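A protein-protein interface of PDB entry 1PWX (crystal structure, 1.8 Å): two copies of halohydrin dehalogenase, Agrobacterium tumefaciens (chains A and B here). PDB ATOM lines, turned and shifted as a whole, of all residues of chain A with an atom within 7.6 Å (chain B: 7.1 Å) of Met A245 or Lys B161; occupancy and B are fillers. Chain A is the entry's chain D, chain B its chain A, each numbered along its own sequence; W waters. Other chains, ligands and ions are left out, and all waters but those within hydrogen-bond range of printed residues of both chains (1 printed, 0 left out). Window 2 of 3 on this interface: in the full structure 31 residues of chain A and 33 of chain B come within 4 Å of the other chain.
The backbone carbonyl oxygen (O) of Ala A207 lies close to the backbone carbonyl oxygen (O) of Gly B164 (3.2 Å). The side-chain amino group (NZ) of Lys B161 sits at hydrogen-bond distance from the backbone carbonyl oxygen (O) of Gly A242, at 3.4 Å. The backbone carbonyl oxygen of Ala A207 lies within hydrogen-bond range of the backbone NH of Glu B165 (3.2 Å).
N of Ala A207 sits close to SD of Met A245 (3.7 Å). N of Ala A207 is in hydrogen-bond range of O of Gly A241. N of Val B170 sits at hydrogen-bond distance from OG1 of Thr B233 (3.1 Å). OG of Ser B160 is in hydrogen-bond range of NZ of Lys B161. O of Gly A241 is in hydrogen-bond range of N of Leu A208. N of Met A245 lies within hydrogen-bond range of O of Val A205, at 2.8 Å.
Among the printed residues, pairs that only touch across the chains: Ala A207 with Ser B160 (3.5 Å), Leu A208 with Thr B233 (3.6 Å), Gly A241 with Thr B233 (3.7 Å), Gly A242 with Thr B233 (3.7 Å), Leu A208 with Gly B164 (3.7 Å), Met A245 with Lys B161 (3.8 Å) and Ala A207 with Lys B161 (3.98 Å).
Of the printed residues of chain B, Ala A207 touches Ser B160 (3.5 Å), Lys B161 (3.98 Å), Gly B164 (2.9 Å) and Glu B165 (3.2 Å). Of the printed residues of chain B, Leu A208 touches Gly B164 (3.7 Å) and Thr B233 (3.6 Å). Printed residues of chain B within 4 Å of Gly A241: Thr B233. Of the printed residues of chain B, Gly A242 touches Lys B161 and Thr B233. Met A245 touches just one residue of chain B: Lys B161 (3.8 Å). Ser B160 touches just one residue of chain A: Ala A207 (3.5 Å). Printed residues of chain A within 4 Å of Gly B164: Ala A207 and Leu A208. The nearest residue of chain B that does not touch Met A245 is Glu B162 (5.8 Å). The nearest printed residue of chain A that does not touch Lys B161 is Pro A244 (4.2 Å).
Of the 16 printed residues of chain A, 5 touch a printed residue of chain B. Printed residues of chain A that touch a printed residue of chain B: Ala A207, Leu A208, Gly A241, Gly A242 and Met A245.
No position is printed for both chains. Of the 10 pairs that touch across the chains among the printed residues, none has its exchanged pair printed and touching as well.
Water W1 lies within hydrogen-bond range of the backbone carbonyl oxygen of Lys B161, the backbone NH of Glu B165 and the backbone carbonyl oxygen of Ala A207.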
ATOM      1  N   PHE A 136       2.616  22.939  24.257  1.00  0.00           N
ATOM      2  CA  PHE A 136       2.070  21.584  24.271  1.00  0.00           C
ATOM      3  C   PHE A 136       3.062  20.572  23.696  1.00  0.00           C
ATOM      4  O   PHE A 136       3.075  19.405  24.082  1.00  0.00           O
ATOM      5  CB  PHE A 136       0.747  21.532  23.492  1.00  0.00           C
ATOM      6  CG  PHE A 136       0.043  20.196  23.574  1.00  0.00           C
ATOM      7  CD1 PHE A 136       0.602  19.053  22.991  1.00  0.00           C
ATOM      8  CD2 PHE A 136      -1.162  20.069  24.267  1.00  0.00           C
ATOM      9  CE1 PHE A 136      -0.025  17.806  23.101  1.00  0.00           C
ATOM     10  CE2 PHE A 136      -1.802  18.815  24.379  1.00  0.00           C
ATOM     11  CZ  PHE A 136      -1.226  17.686  23.794  1.00  0.00           C
ATOM     12  N   LYS A 203       3.616  18.633   6.744  1.00  0.00           N
ATOM     13  CA  LYS A 203       2.791  17.523   6.272  1.00  0.00           C
ATOM     14  C   LYS A 203       3.044  16.286   7.126  1.00  0.00           C
ATOM     15  O   LYS A 203       2.482  15.227   6.864  1.00  0.00           O
ATOM     16  CB  LYS A 203       3.166  17.204   4.817  1.00  0.00           C
ATOM     17  CG  LYS A 203       2.429  16.036   4.186  1.00  0.00           C
ATOM     18  CD  LYS A 203       0.977  16.372   3.881  1.00  0.00           C
ATOM     19  CE  LYS A 203       0.849  17.476   2.842  1.00  0.00           C
ATOM     20  NZ  LYS A 203      -0.569  17.728   2.482  1.00  0.00           N
ATOM     21  N   LYS A 204       3.866  16.430   8.161  1.00  0.00           N
ATOM     22  CA  LYS A 204       4.230  15.290   9.002  1.00  0.00           C
ATOM     23  C   LYS A 204       3.868  15.332  10.496  1.00  0.00           C
ATOM     24  O   LYS A 204       3.373  14.348  11.049  1.00  0.00           O
ATOM     25  CB  LYS A 204       5.738  15.037   8.837  1.00  0.00           C
ATOM     26  CG  LYS A 204       6.319  13.950   9.725  1.00  0.00           C
ATOM     27  CD  LYS A 204       7.091  14.545  10.903  1.00  0.00           C
ATOM     28  CE  LYS A 204       7.951  13.476  11.568  1.00  0.00           C
ATOM     29  NZ  LYS A 204       8.902  13.986  12.592  1.00  0.00           N
ATOM     30  N   VAL A 205       4.126  16.454  11.153  1.00  0.00           N
ATOM     31  CA  VAL A 205       3.827  16.567  12.575  1.00  0.00           C
ATOM     32  C   VAL A 205       2.337  16.770  12.874  1.00  0.00           C
ATOM     33  O   VAL A 205       1.944  16.847  14.042  1.00  0.00           O
ATOM     34  CB  VAL A 205       4.637  17.713  13.228  1.00  0.00           C
ATOM     35  CG1 VAL A 205       5.810  17.134  14.035  1.00  0.00           C
ATOM     36  CG2 VAL A 205       5.148  18.661  12.162  1.00  0.00           C
ATOM     37  N   THR A 206       1.514  16.855  11.825  1.00  0.00           N
ATOM     38  CA  THR A 206       0.071  17.035  11.998  1.00  0.00           C
ATOM     39  C   THR A 206      -0.752  15.838  11.509  1.00  0.00           C
ATOM     40  O   THR A 206      -0.420  15.225  10.491  1.00  0.00           O
ATOM     41  CB  THR A 206      -0.455  18.312  11.255  1.00  0.00           C
ATOM     42  OG1 THR A 206       0.032  18.332   9.905  1.00  0.00           O
ATOM     43  CG2 THR A 206      -0.022  19.576  11.969  1.00  0.00           C
ATOM     44  N   ALA A 207      -1.828  15.515  12.226  1.00  0.00           N
ATOM     45  CA  ALA A 207      -2.706  14.408  11.842  1.00  0.00           C
ATOM     46  C   ALA A 207      -3.476  14.697  10.542  1.00  0.00           C
ATOM     47  O   ALA A 207      -3.904  13.772   9.849  1.00  0.00           O
ATOM     48  CB  ALA A 207      -3.687  14.106  12.964  1.00  0.00           C
ATOM     49  N   LEU A 208      -3.650  15.980  10.224  1.00  0.00           N
ATOM     50  CA  LEU A 208      -4.353  16.415   9.012  1.00  0.00           C
ATOM     51  C   LEU A 208      -3.399  16.673   7.837  1.00  0.00           C
ATOM     52  O   LEU A 208      -3.834  16.803   6.688  1.00  0.00           O
ATOM     53  CB  LEU A 208      -5.161  17.686   9.300  1.00  0.00           C
ATOM     54  CG  LEU A 208      -6.455  17.432  10.063  1.00  0.00           C
ATOM     55  CD1 LEU A 208      -7.059  18.743  10.545  1.00  0.00           C
ATOM     56  CD2 LEU A 208      -7.411  16.676   9.142  1.00  0.00           C
ATOM     57  N   GLN A 209      -2.104  16.752   8.135  1.00  0.00           N
ATOM     58  CA  GLN A 209      -1.080  16.980   7.121  1.00  0.00           C
ATOM     59  C   GLN A 209      -1.278  18.249   6.295  1.00  0.00           C
ATOM     60  O   GLN A 209      -1.436  18.197   5.077  1.00  0.00           O
ATOM     61  CB  GLN A 209      -1.008  15.787   6.164  1.00  0.00           C
ATOM     62  CG  GLN A 209      -1.159  14.423   6.805  1.00  0.00           C
ATOM     63  CD  GLN A 209      -0.941  13.316   5.806  1.00  0.00           C
ATOM     64  OE1 GLN A 209      -1.202  13.486   4.608  1.00  0.00           O
ATOM     65  NE2 GLN A 209      -0.469  12.165   6.288  1.00  0.00           N
ATOM     66  N   GLY A 241      -4.269  21.357  14.212  1.00  0.00           N
ATOM     67  CA  GLY A 241      -4.670  20.321  13.279  1.00  0.00           C
ATOM     68  C   GLY A 241      -4.157  18.921  13.553  1.00  0.00           C
ATOM     69  O   GLY A 241      -3.851  18.163  12.623  1.00  0.00           O
ATOM     70  N   GLY A 242      -4.075  18.567  14.829  1.00  0.00           N
ATOM     71  CA  GLY A 242      -3.602  17.248  15.186  1.00  0.00           C
ATOM     72  C   GLY A 242      -2.168  17.224  15.675  1.00  0.00           C
ATOM     73  O   GLY A 242      -1.710  16.212  16.206  1.00  0.00           O
ATOM     74  N   PHE A 243      -1.454  18.328  15.496  1.00  0.00           N
ATOM     75  CA  PHE A 243      -0.073  18.409  15.950  1.00  0.00           C
ATOM     76  C   PHE A 243       0.010  18.062  17.438  1.00  0.00           C
ATOM     77  O   PHE A 243      -0.816  18.508  18.238  1.00  0.00           O
ATOM     78  CB  PHE A 243       0.460  19.817  15.688  1.00  0.00           C
ATOM     79  CG  PHE A 243       1.638  20.210  16.550  1.00  0.00           C
ATOM     80  CD1 PHE A 243       1.441  20.801  17.795  1.00  0.00           C
ATOM     81  CD2 PHE A 243       2.946  20.011  16.105  1.00  0.00           C
ATOM     82  CE1 PHE A 243       2.530  21.190  18.584  1.00  0.00           C
ATOM     83  CE2 PHE A 243       4.029  20.392  16.880  1.00  0.00           C
ATOM     84  CZ  PHE A 243       3.824  20.985  18.124  1.00  0.00           C
ATOM     85  N   PRO A 244       1.010  17.259  17.829  1.00  0.00           N
ATOM     86  CA  PRO A 244       2.022  16.689  16.941  1.00  0.00           C
ATOM     87  C   PRO A 244       1.782  15.199  16.701  1.00  0.00           C
ATOM     88  O   PRO A 244       1.014  14.559  17.412  1.00  0.00           O
ATOM     89  CB  PRO A 244       3.296  16.923  17.722  1.00  0.00           C
ATOM     90  CG  PRO A 244       2.839  16.545  19.136  1.00  0.00           C
ATOM     91  CD  PRO A 244       1.416  17.098  19.239  1.00  0.00           C
ATOM     92  N   MET A 245       2.430  14.664  15.680  1.00  0.00           N
ATOM     93  CA  MET A 245       2.340  13.249  15.380  1.00  0.00           C
ATOM     94  C   MET A 245       3.622  12.727  16.013  1.00  0.00           C
ATOM     95  O   MET A 245       4.710  13.195  15.694  1.00  0.00           O
ATOM     96  CB  MET A 245       2.354  12.996  13.866  1.00  0.00           C
ATOM     97  CG  MET A 245       1.072  13.353  13.116  1.00  0.00           C
ATOM     98  SD  MET A 245      -0.380  12.392  13.614  1.00  0.00           S
ATOM     99  CE  MET A 245      -0.125  10.883  12.725  1.00  0.00           C
ATOM    100  N   ILE A 246       3.504  11.768  16.920  1.00  0.00           N
ATOM    101  CA  ILE A 246       4.686  11.257  17.591  1.00  0.00           C
ATOM    102  C   ILE A 246       5.363  10.129  16.831  1.00  0.00           C
ATOM    103  O   ILE A 246       4.725   9.176  16.385  1.00  0.00           O
ATOM    104  CB  ILE A 246       4.352  10.788  19.041  1.00  0.00           C
ATOM    105  CG1 ILE A 246       3.821  11.968  19.873  1.00  0.00           C
ATOM    106  CG2 ILE A 246       5.597  10.217  19.703  1.00  0.00           C
ATOM    107  CD1 ILE A 246       2.373  12.352  19.580  1.00  0.00           C
ATOM    108  N   GLU A 247       6.670  10.268  16.672  1.00  0.00           N
ATOM    109  CA  GLU A 247       7.477   9.277  15.991  1.00  0.00           C
ATOM    110  C   GLU A 247       7.147   7.870  16.518  1.00  0.00           C
ATOM    111  O   GLU A 247       7.480   7.533  17.660  1.00  0.00           O
ATOM    112  CB  GLU A 247       8.960   9.587  16.232  1.00  0.00           C
ATOM    113  CG  GLU A 247       9.920   8.889  15.277  1.00  0.00           C
ATOM    114  CD  GLU A 247       9.984   9.552  13.918  1.00  0.00           C
ATOM    115  OE1 GLU A 247      10.324   8.848  12.929  1.00  0.00           O
ATOM    116  OE2 GLU A 247       9.709  10.777  13.838  1.00  0.00           O
ATOM    117  N   ARG A 248       6.474   7.061  15.703  1.00  0.00           N
ATOM    118  CA  ARG A 248       6.163   5.699  16.117  1.00  0.00           C
ATOM    119  C   ARG A 248       7.482   4.949  16.138  1.00  0.00           C
ATOM    120  O   ARG A 248       8.506   5.466  15.685  1.00  0.00           O
ATOM    121  CB  ARG A 248       5.210   5.020  15.136  1.00  0.00           C
ATOM    122  CG  ARG A 248       3.747   5.313  15.401  1.00  0.00           C
ATOM    123  CD  ARG A 248       2.867   4.507  14.488  1.00  0.00           C
ATOM    124  NE  ARG A 248       3.008   4.908  13.098  1.00  0.00           N
ATOM    125  CZ  ARG A 248       2.653   4.144  12.070  1.00  0.00           C
ATOM    126  NH1 ARG A 248       2.141   2.936  12.281  1.00  0.00           N
ATOM    127  NH2 ARG A 248       2.792   4.590  10.831  1.00  0.00           N
ATOM    128  N   LEU B 155      -9.800   8.773  24.304  1.00  0.00           N
ATOM    129  CA  LEU B 155     -10.046   7.955  23.123  1.00  0.00           C
ATOM    130  C   LEU B 155     -10.351   8.901  21.952  1.00  0.00           C
ATOM    131  O   LEU B 155      -9.911   8.687  20.821  1.00  0.00           O
ATOM    132  CB  LEU B 155     -11.220   7.012  23.400  1.00  0.00           C
ATOM    133  CG  LEU B 155     -11.694   5.990  22.360  1.00  0.00           C
ATOM    134  CD1 LEU B 155     -12.739   6.633  21.494  1.00  0.00           C
ATOM    135  CD2 LEU B 155     -10.525   5.438  21.538  1.00  0.00           C
ATOM    136  N   ALA B 156     -11.089   9.968  22.242  1.00  0.00           N
ATOM    137  CA  ALA B 156     -11.444  10.958  21.225  1.00  0.00           C
ATOM    138  C   ALA B 156     -10.173  11.570  20.651  1.00  0.00           C
ATOM    139  O   ALA B 156     -10.000  11.629  19.447  1.00  0.00           O
ATOM    140  CB  ALA B 156     -12.305  12.041  21.837  1.00  0.00           C
ATOM    141  N   ASN B 157      -9.284  12.013  21.532  1.00  0.00           N
ATOM    142  CA  ASN B 157      -8.024  12.620  21.117  1.00  0.00           C
ATOM    143  C   ASN B 157      -7.123  11.601  20.406  1.00  0.00           C
ATOM    144  O   ASN B 157      -6.485  11.911  19.406  1.00  0.00           O
ATOM    145  CB  ASN B 157      -7.332  13.228  22.344  1.00  0.00           C
ATOM    146  CG  ASN B 157      -5.900  13.633  22.073  1.00  0.00           C
ATOM    147  OD1 ASN B 157      -4.975  12.875  22.351  1.00  0.00           O
ATOM    148  ND2 ASN B 157      -5.709  14.833  21.526  1.00  0.00           N
ATOM    149  N   ALA B 158      -7.084  10.379  20.918  1.00  0.00           N
ATOM    150  CA  ALA B 158      -6.285   9.333  20.296  1.00  0.00           C
ATOM    151  C   ALA B 158      -6.778   9.119  18.872  1.00  0.00           C
ATOM    152  O   ALA B 158      -6.001   9.224  17.930  1.00  0.00           O
ATOM    153  CB  ALA B 158      -6.387   8.026  21.103  1.00  0.00           C
ATOM    154  N   LEU B 159      -8.072   8.842  18.712  1.00  0.00           N
ATOM    155  CA  LEU B 159      -8.651   8.618  17.382  1.00  0.00           C
ATOM    156  C   LEU B 159      -8.348   9.725  16.366  1.00  0.00           C
ATOM    157  O   LEU B 159      -8.287   9.480  15.160  1.00  0.00           O
ATOM    158  CB  LEU B 159     -10.161   8.448  17.487  1.00  0.00           C
ATOM    159  CG  LEU B 159     -10.716   7.136  18.032  1.00  0.00           C
ATOM    160  CD1 LEU B 159     -12.237   7.231  18.180  1.00  0.00           C
ATOM    161  CD2 LEU B 159     -10.333   5.997  17.094  1.00  0.00           C
ATOM    162  N   SER B 160      -8.170  10.946  16.855  1.00  0.00           N
ATOM    163  CA  SER B 160      -7.879  12.076  15.993  1.00  0.00           C
ATOM    164  C   SER B 160      -6.572  11.788  15.266  1.00  0.00           C
ATOM    165  O   SER B 160      -6.374  12.192  14.119  1.00  0.00           O
ATOM    166  CB  SER B 160      -7.749  13.355  16.822  1.00  0.00           C
ATOM    167  OG  SER B 160      -6.571  13.349  17.608  1.00  0.00           O
ATOM    168  N   LYS B 161      -5.699  11.066  15.959  1.00  0.00           N
ATOM    169  CA  LYS B 161      -4.391  10.681  15.455  1.00  0.00           C
ATOM    170  C   LYS B 161      -4.480   9.840  14.188  1.00  0.00           C
ATOM    171  O   LYS B 161      -3.816  10.132  13.192  1.00  0.00           O
ATOM    172  CB  LYS B 161      -3.641   9.908  16.550  1.00  0.00           C
ATOM    173  CG  LYS B 161      -3.455  10.722  17.834  1.00  0.00           C
ATOM    174  CD  LYS B 161      -2.493  11.888  17.576  1.00  0.00           C
ATOM    175  CE  LYS B 161      -2.796  13.099  18.454  1.00  0.00           C
ATOM    176  NZ  LYS B 161      -3.776  14.017  17.800  1.00  0.00           N
ATOM    177  N   GLU B 162      -5.302   8.798  14.219  1.00  0.00           N
ATOM    178  CA  GLU B 162      -5.424   7.930  13.060  1.00  0.00           C
ATOM    179  C   GLU B 162      -6.480   8.363  12.062  1.00  0.00           C
ATOM    180  O   GLU B 162      -6.384   8.034  10.889  1.00  0.00           O
ATOM    181  CB  GLU B 162      -5.710   6.491  13.491  1.00  0.00           C
ATOM    182  CG  GLU B 162      -6.998   6.339  14.268  1.00  0.00           C
ATOM    183  CD  GLU B 162      -7.308   4.896  14.588  1.00  0.00           C
ATOM    184  OE1 GLU B 162      -7.570   4.135  13.636  1.00  0.00           O
ATOM    185  OE2 GLU B 162      -7.294   4.523  15.781  1.00  0.00           O
ATOM    186  N   LEU B 163      -7.484   9.112  12.504  1.00  0.00           N
ATOM    187  CA  LEU B 163      -8.543   9.507  11.580  1.00  0.00           C
ATOM    188  C   LEU B 163      -8.277  10.736  10.692  1.00  0.00           C
ATOM    189  O   LEU B 163      -8.845  10.847   9.610  1.00  0.00           O
ATOM    190  CB  LEU B 163      -9.876   9.612  12.348  1.00  0.00           C
ATOM    191  CG  LEU B 163     -10.266   8.278  13.032  1.00  0.00           C
ATOM    192  CD1 LEU B 163     -11.675   8.366  13.614  1.00  0.00           C
ATOM    193  CD2 LEU B 163     -10.200   7.133  12.025  1.00  0.00           C
ATOM    194  N   GLY B 164      -7.387  11.620  11.123  1.00  0.00           N
ATOM    195  CA  GLY B 164      -7.059  12.796  10.327  1.00  0.00           C
ATOM    196  C   GLY B 164      -6.389  12.475   8.996  1.00  0.00           C
ATOM    197  O   GLY B 164      -6.478  13.248   8.042  1.00  0.00           O
ATOM    198  N   GLU B 165      -5.713  11.333   8.932  1.00  0.00           N
ATOM    199  CA  GLU B 165      -5.045  10.881   7.712  1.00  0.00           C
ATOM    200  C   GLU B 165      -6.055  10.753   6.569  1.00  0.00           C
ATOM    201  O   GLU B 165      -5.688  10.724   5.383  1.00  0.00           O
ATOM    202  CB  GLU B 165      -4.386   9.531   7.961  1.00  0.00           C
ATOM    203  CG  GLU B 165      -4.105   8.737   6.713  1.00  0.00           C
ATOM    204  CD  GLU B 165      -3.227   7.553   6.996  1.00  0.00           C
ATOM    205  OE1 GLU B 165      -3.284   6.571   6.227  1.00  0.00           O
ATOM    206  OE2 GLU B 165      -2.469   7.607   7.988  1.00  0.00           O
ATOM    207  N   ILE B 168     -10.681  13.243   8.711  1.00  0.00           N
ATOM    208  CA  ILE B 168     -11.825  13.082   9.618  1.00  0.00           C
ATOM    209  C   ILE B 168     -11.569  13.650  11.019  1.00  0.00           C
ATOM    210  O   ILE B 168     -10.824  13.068  11.803  1.00  0.00           O
ATOM    211  CB  ILE B 168     -12.194  11.581   9.769  1.00  0.00           C
ATOM    212  CG1 ILE B 168     -12.536  10.990   8.392  1.00  0.00           C
ATOM    213  CG2 ILE B 168     -13.360  11.423  10.742  1.00  0.00           C
ATOM    214  CD1 ILE B 168     -12.455   9.468   8.330  1.00  0.00           C
ATOM    215  N   VAL B 170     -12.037  14.573  14.955  1.00  0.00           N
ATOM    216  CA  VAL B 170     -12.580  13.872  16.107  1.00  0.00           C
ATOM    217  C   VAL B 170     -12.380  14.769  17.325  1.00  0.00           C
ATOM    218  O   VAL B 170     -11.262  15.153  17.647  1.00  0.00           O
ATOM    219  CB  VAL B 170     -11.880  12.515  16.325  1.00  0.00           C
ATOM    220  CG1 VAL B 170     -12.486  11.803  17.529  1.00  0.00           C
ATOM    221  CG2 VAL B 170     -12.044  11.639  15.068  1.00  0.00           C
ATOM    222  N   THR B 233      -9.232  19.409  15.478  1.00  0.00           N
ATOM    223  CA  THR B 233      -9.263  17.960  15.672  1.00  0.00           C
ATOM    224  C   THR B 233      -8.300  17.468  16.757  1.00  0.00           C
ATOM    225  O   THR B 233      -7.122  17.820  16.775  1.00  0.00           O
ATOM    226  CB  THR B 233      -8.969  17.205  14.353  1.00  0.00           C
ATOM    227  OG1 THR B 233      -9.197  15.803  14.551  1.00  0.00           O
ATOM    228  CG2 THR B 233      -7.524  17.447  13.894  1.00  0.00           C
ATOM    229  N   GLY B 234      -8.827  16.653  17.661  1.00  0.00           N
ATOM    230  CA  GLY B 234      -8.036  16.135  18.759  1.00  0.00           C
ATOM    231  C   GLY B 234      -8.268  16.999  19.986  1.00  0.00           C
ATOM    232  O   GLY B 234      -7.642  16.801  21.022  1.00  0.00           O
ATOM    233  N   GLN B 235      -9.184  17.955  19.867  1.00  0.00           N
ATOM    234  CA  GLN B 235      -9.490  18.876  20.958  1.00  0.00           C
ATOM    235  C   GLN B 235     -10.618  18.464  21.892  1.00  0.00           C
ATOM    236  O   GLN B 235     -11.650  17.948  21.462  1.00  0.00           O
ATOM    237  CB  GLN B 235      -9.825  20.261  20.393  1.00  0.00           C
ATOM    238  CG  GLN B 235     -10.203  21.300  21.439  1.00  0.00           C
ATOM    239  CD  GLN B 235      -9.008  22.098  21.938  1.00  0.00           C
ATOM    240  OE1 GLN B 235      -8.265  22.684  21.146  1.00  0.00           O
ATOM    241  NE2 GLN B 235      -8.827  22.137  23.260  1.00  0.00           N
HETATM  242  O   HOH W   1      -3.792  10.839  10.803  1.00  0.00           O
